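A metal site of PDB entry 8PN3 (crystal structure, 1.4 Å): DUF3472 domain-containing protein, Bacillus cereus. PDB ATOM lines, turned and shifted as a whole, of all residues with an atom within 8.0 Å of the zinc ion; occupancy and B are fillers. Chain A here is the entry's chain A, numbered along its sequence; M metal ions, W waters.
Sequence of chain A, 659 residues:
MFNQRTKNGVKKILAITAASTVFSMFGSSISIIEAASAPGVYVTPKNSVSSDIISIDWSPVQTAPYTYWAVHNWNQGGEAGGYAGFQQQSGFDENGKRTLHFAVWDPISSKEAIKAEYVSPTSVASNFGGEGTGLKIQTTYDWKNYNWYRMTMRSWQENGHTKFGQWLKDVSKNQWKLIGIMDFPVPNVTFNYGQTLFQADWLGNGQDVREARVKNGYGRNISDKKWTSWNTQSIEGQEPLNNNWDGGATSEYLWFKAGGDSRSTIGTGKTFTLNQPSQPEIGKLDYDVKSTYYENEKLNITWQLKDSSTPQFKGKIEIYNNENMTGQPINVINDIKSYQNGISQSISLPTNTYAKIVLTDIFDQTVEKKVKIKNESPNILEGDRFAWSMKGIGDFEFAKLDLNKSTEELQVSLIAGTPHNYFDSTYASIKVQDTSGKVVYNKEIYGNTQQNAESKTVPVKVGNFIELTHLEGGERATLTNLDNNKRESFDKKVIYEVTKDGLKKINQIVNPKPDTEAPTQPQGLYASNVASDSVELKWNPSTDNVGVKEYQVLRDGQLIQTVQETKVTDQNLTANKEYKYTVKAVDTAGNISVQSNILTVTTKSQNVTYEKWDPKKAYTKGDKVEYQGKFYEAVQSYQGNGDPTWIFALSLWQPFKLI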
ATOM      1  N   GLU A 117     -17.370  19.145  26.163  1.00  0.00           N
ATOM      2  CA  GLU A 117     -18.179  17.942  26.279  1.00  0.00           C
ATOM      3  C   GLU A 117     -17.369  16.752  26.750  1.00  0.00           C
ATOM      4  O   GLU A 117     -17.862  15.931  27.500  1.00  0.00           O
ATOM      5  CB  GLU A 117     -18.838  17.652  24.944  1.00  0.00           C
ATOM      6  CG  GLU A 117     -19.751  16.449  24.998  1.00  0.00           C
ATOM      7  CD  GLU A 117     -20.508  16.205  23.709  1.00  0.00           C
ATOM      8  OE1 GLU A 117     -21.003  17.200  23.122  1.00  0.00           O
ATOM      9  OE2 GLU A 117     -20.555  15.059  23.283  1.00  0.00           O
ATOM     10  N   TRP A 156     -19.403  18.675  13.391  1.00  0.00           N
ATOM     11  CA  TRP A 156     -20.688  18.116  12.998  1.00  0.00           C
ATOM     12  C   TRP A 156     -21.831  18.898  13.636  1.00  0.00           C
ATOM     13  O   TRP A 156     -21.661  19.503  14.680  1.00  0.00           O
ATOM     14  CB  TRP A 156     -20.818  16.620  13.287  1.00  0.00           C
ATOM     15  CG  TRP A 156     -20.737  16.187  14.717  1.00  0.00           C
ATOM     16  CD1 TRP A 156     -21.804  15.832  15.511  1.00  0.00           C
ATOM     17  CD2 TRP A 156     -19.545  16.023  15.538  1.00  0.00           C
ATOM     18  NE1 TRP A 156     -21.341  15.464  16.732  1.00  0.00           N
ATOM     19  CE2 TRP A 156     -19.966  15.523  16.777  1.00  0.00           C
ATOM     20  CE3 TRP A 156     -18.175  16.182  15.330  1.00  0.00           C
ATOM     21  CZ2 TRP A 156     -19.070  15.231  17.821  1.00  0.00           C
ATOM     22  CZ3 TRP A 156     -17.293  15.909  16.334  1.00  0.00           C
ATOM     23  CH2 TRP A 156     -17.727  15.407  17.576  1.00  0.00           C
ATOM     24  N   GLN A 157     -23.026  18.766  13.045  1.00  0.00           N
ATOM     25  CA  GLN A 157     -24.230  19.397  13.579  1.00  0.00           C
ATOM     26  C   GLN A 157     -24.909  18.453  14.548  1.00  0.00           C
ATOM     27  O   GLN A 157     -25.078  17.256  14.275  1.00  0.00           O
ATOM     28  CB  GLN A 157     -25.193  19.731  12.457  1.00  0.00           C
ATOM     29  CG  GLN A 157     -24.607  20.697  11.439  1.00  0.00           C
ATOM     30  CD  GLN A 157     -24.186  21.978  12.103  1.00  0.00           C
ATOM     31  OE1 GLN A 157     -22.988  22.293  12.310  1.00  0.00           O
ATOM     32  NE2 GLN A 157     -25.196  22.715  12.526  1.00  0.00           N
ATOM     33  N   GLU A 158     -25.347  18.977  15.688  1.00  0.00           N
ATOM     34  CA  GLU A 158     -26.110  18.161  16.598  1.00  0.00           C
ATOM     35  C   GLU A 158     -26.898  19.060  17.530  1.00  0.00           C
ATOM     36  O   GLU A 158     -26.330  19.978  18.131  1.00  0.00           O
ATOM     37  CB  GLU A 158     -25.148  17.294  17.393  1.00  0.00           C
ATOM     38  CG  GLU A 158     -25.851  16.242  18.206  1.00  0.00           C
ATOM     39  CD  GLU A 158     -24.943  15.174  18.749  1.00  0.00           C
ATOM     40  OE1 GLU A 158     -23.707  15.359  18.880  1.00  0.00           O
ATOM     41  OE2 GLU A 158     -25.518  14.071  18.977  1.00  0.00           O
ATOM     42  N   ASN A 159     -28.202  18.789  17.647  1.00  0.00           N
ATOM     43  CA  ASN A 159     -29.032  19.465  18.659  1.00  0.00           C
ATOM     44  C   ASN A 159     -29.042  20.982  18.470  1.00  0.00           C
ATOM     45  O   ASN A 159     -29.168  21.716  19.450  1.00  0.00           O
ATOM     46  CB  ASN A 159     -28.638  19.006  20.057  1.00  0.00           C
ATOM     47  CG  ASN A 159     -28.813  17.520  20.356  1.00  0.00           C
ATOM     48  OD1 ASN A 159     -27.956  16.898  20.976  1.00  0.00           O
ATOM     49  ND2 ASN A 159     -29.931  16.959  19.966  1.00  0.00           N
ATOM     50  N   LYS A 163     -20.554  20.719  16.973  1.00  0.00           N
ATOM     51  CA  LYS A 163     -19.477  20.118  17.751  1.00  0.00           C
ATOM     52  C   LYS A 163     -18.171  20.159  16.960  1.00  0.00           C
ATOM     53  O   LYS A 163     -18.211  20.113  15.747  1.00  0.00           O
ATOM     54  CB  LYS A 163     -19.808  18.658  18.024  1.00  0.00           C
ATOM     55  CG  LYS A 163     -21.172  18.377  18.658  1.00  0.00           C
ATOM     56  CD  LYS A 163     -21.413  19.061  19.949  1.00  0.00           C
ATOM     57  CE  LYS A 163     -22.768  18.763  20.574  1.00  0.00           C
ATOM     58  NZ  LYS A 163     -22.847  17.361  21.018  1.00  0.00           N
ATOM     59  N   PHE A 313     -16.723   7.242  16.176  1.00  0.00           N
ATOM     60  CA  PHE A 313     -17.448   8.504  16.137  1.00  0.00           C
ATOM     61  C   PHE A 313     -18.789   8.397  16.870  1.00  0.00           C
ATOM     62  O   PHE A 313     -19.146   9.284  17.674  1.00  0.00           O
ATOM     63  CB  PHE A 313     -17.617   8.899  14.669  1.00  0.00           C
ATOM     64  CG  PHE A 313     -18.294  10.239  14.415  1.00  0.00           C
ATOM     65  CD1 PHE A 313     -17.786  11.402  14.998  1.00  0.00           C
ATOM     66  CD2 PHE A 313     -19.452  10.322  13.679  1.00  0.00           C
ATOM     67  CE1 PHE A 313     -18.395  12.614  14.733  1.00  0.00           C
ATOM     68  CE2 PHE A 313     -20.073  11.541  13.432  1.00  0.00           C
ATOM     69  CZ  PHE A 313     -19.540  12.684  13.943  1.00  0.00           C
ATOM     70  N   LYS A 314     -19.549   7.306  16.589  1.00  0.00           N
ATOM     71  CA  LYS A 314     -20.880   7.161  17.167  1.00  0.00           C
ATOM     72  C   LYS A 314     -21.289   5.696  17.109  1.00  0.00           C
ATOM     73  O   LYS A 314     -20.740   4.923  16.346  1.00  0.00           O
ATOM     74  CB  LYS A 314     -21.897   8.058  16.487  1.00  0.00           C
ATOM     75  CG  LYS A 314     -22.193   7.719  15.048  1.00  0.00           C
ATOM     76  CD  LYS A 314     -23.206   8.629  14.339  1.00  0.00           C
ATOM     77  CE  LYS A 314     -23.301   8.205  12.893  1.00  0.00           C
ATOM     78  NZ  LYS A 314     -24.296   9.007  12.171  1.00  0.00           N
ATOM     79  N   GLY A 315     -22.264   5.359  17.960  1.00  0.00           N
ATOM     80  CA  GLY A 315     -22.852   4.041  17.970  1.00  0.00           C
ATOM     81  C   GLY A 315     -24.366   4.089  18.114  1.00  0.00           C
ATOM     82  O   GLY A 315     -24.934   5.097  18.549  1.00  0.00           O
ATOM     83  N   ASN A 334     -29.997   5.077  20.955  1.00  0.00           N
ATOM     84  CA  ASN A 334     -29.399   6.020  20.021  1.00  0.00           C
ATOM     85  C   ASN A 334     -28.284   6.851  20.655  1.00  0.00           C
ATOM     86  O   ASN A 334     -28.148   6.971  21.883  1.00  0.00           O
ATOM     87  CB  ASN A 334     -30.481   6.965  19.467  1.00  0.00           C
ATOM     88  CG  ASN A 334     -31.394   6.300  18.480  1.00  0.00           C
ATOM     89  OD1 ASN A 334     -30.917   5.743  17.497  1.00  0.00           O
ATOM     90  ND2 ASN A 334     -32.683   6.330  18.765  1.00  0.00           N
ATOM     91  N   ASP A 335     -27.465   7.401  19.757  1.00  0.00           N
ATOM     92  CA  ASP A 335     -26.538   8.465  20.105  1.00  0.00           C
ATOM     93  C   ASP A 335     -25.540   8.041  21.181  1.00  0.00           C
ATOM     94  O   ASP A 335     -25.262   8.751  22.135  1.00  0.00           O
ATOM     95  CB  ASP A 335     -27.283   9.752  20.508  1.00  0.00           C
ATOM     96  CG  ASP A 335     -26.402  10.983  20.535  1.00  0.00           C
ATOM     97  OD1 ASP A 335     -25.364  10.975  19.823  1.00  0.00           O
ATOM     98  OD2 ASP A 335     -26.693  11.916  21.353  1.00  0.00           O
ATOM     99  N   ILE A 336     -24.963   6.862  21.011  1.00  0.00           N
ATOM    100  CA  ILE A 336     -23.839   6.425  21.816  1.00  0.00           C
ATOM    101  C   ILE A 336     -22.633   7.203  21.335  1.00  0.00           C
ATOM    102  O   ILE A 336     -22.344   7.246  20.123  1.00  0.00           O
ATOM    103  CB  ILE A 336     -23.666   4.897  21.710  1.00  0.00           C
ATOM    104  CG1 ILE A 336     -24.936   4.167  22.162  1.00  0.00           C
ATOM    105  CG2 ILE A 336     -22.474   4.454  22.542  1.00  0.00           C
ATOM    106  CD1 ILE A 336     -24.998   2.736  21.773  1.00  0.00           C
ATOM    107  N   LYS A 337     -21.938   7.861  22.252  1.00  0.00           N
ATOM    108  CA  LYS A 337     -20.936   8.842  21.860  1.00  0.00           C
ATOM    109  C   LYS A 337     -19.608   8.197  21.514  1.00  0.00           C
ATOM    110  O   LYS A 337     -19.347   7.022  21.806  1.00  0.00           O
ATOM    111  CB  LYS A 337     -20.775   9.807  23.035  1.00  0.00           C
ATOM    112  CG  LYS A 337     -22.036  10.581  23.389  1.00  0.00           C
ATOM    113  CD  LYS A 337     -22.373  11.559  22.290  1.00  0.00           C
ATOM    114  CE  LYS A 337     -23.566  12.423  22.621  1.00  0.00           C
ATOM    115  NZ  LYS A 337     -23.830  13.416  21.556  1.00  0.00           N
ATOM    116  N   SER A 338     -18.706   9.003  20.919  1.00  0.00           N
ATOM    117  CA  SER A 338     -17.371   8.553  20.595  1.00  0.00           C
ATOM    118  C   SER A 338     -16.642   7.982  21.800  1.00  0.00           C
ATOM    119  O   SER A 338     -15.827   7.054  21.669  1.00  0.00           O
ATOM    120  CB  SER A 338     -16.554   9.658  20.003  1.00  0.00           C
ATOM    121  OG  SER A 338     -16.620  10.798  20.856  1.00  0.00           O
ATOM    122  N   TYR A 339     -16.944   8.558  22.973  1.00  0.00           N
ATOM    123  CA  TYR A 339     -16.258   8.292  24.229  1.00  0.00           C
ATOM    124  C   TYR A 339     -17.027   7.282  25.094  1.00  0.00           C
ATOM    125  O   TYR A 339     -16.738   7.151  26.311  1.00  0.00           O
ATOM    126  CB  TYR A 339     -16.024   9.604  24.990  1.00  0.00           C
ATOM    127  CG  TYR A 339     -17.189  10.548  25.024  1.00  0.00           C
ATOM    128  CD1 TYR A 339     -18.213  10.439  25.978  1.00  0.00           C
ATOM    129  CD2 TYR A 339     -17.309  11.554  24.105  1.00  0.00           C
ATOM    130  CE1 TYR A 339     -19.300  11.302  25.970  1.00  0.00           C
ATOM    131  CE2 TYR A 339     -18.365  12.445  24.098  1.00  0.00           C
ATOM    132  CZ  TYR A 339     -19.355  12.344  25.051  1.00  0.00           C
ATOM    133  OH  TYR A 339     -20.445  13.186  25.037  1.00  0.00           O
ATOM    134  N   GLN A 340     -17.984   6.548  24.503  1.00  0.00           N
ATOM    135  CA  GLN A 340     -18.723   5.495  25.200  1.00  0.00           C
ATOM    136  C   GLN A 340     -18.551   4.165  24.486  1.00  0.00           C
ATOM    137  O   GLN A 340     -18.782   4.083  23.282  1.00  0.00           O
ATOM    138  CB  GLN A 340     -20.188   5.877  25.315  1.00  0.00           C
ATOM    139  CG  GLN A 340     -20.399   7.102  26.219  1.00  0.00           C
ATOM    140  CD  GLN A 340     -21.712   7.819  26.047  1.00  0.00           C
ATOM    141  OE1 GLN A 340     -22.471   7.559  25.107  1.00  0.00           O
ATOM    142  NE2 GLN A 340     -21.958   8.798  26.949  1.00  0.00           N
HETATM  143 ZN    ZN M   1     -24.289  12.716  19.708  1.00  0.00          ZN
HETATM  144  O   HOH W   1     -21.462  12.486  19.023  1.00  0.00           O
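The side-chain carboxylate (OE1) of Glu 158 sits at hydrogen-bond distance from the indole nitrogen (NE1) of Trp 156 (3.2 Å). NZ of Lys 163 is in salt-bridge range of OE1 of Glu 158, at 3.1 Å. The backbone NH (N) of Lys 337 lies within hydrogen-bond range of the side-chain amide oxygen (OE1) of Gln 340 (2.9 Å).
Three residues have an atom within 4 Å of the zinc ion: Glu 158, Asp 335 and Lys 337. The nearest printed residue that does not touch the zinc ion is Trp 156 (5.0 Å).
The side-chain carboxylate (OE2) of Glu 158 binds the zinc ion, at 2.0 Å. The zinc ion is bound by the side-chain amino group (NZ) of Lys 337 (2.0 Å). The side-chain carboxylate (OD1) of Asp 335 is bound to the zinc ion. The zinc ion has three donor atoms within binding distance. Slightly farther from the zinc ion lies OE1 of Glu 158 (2.8 Å).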
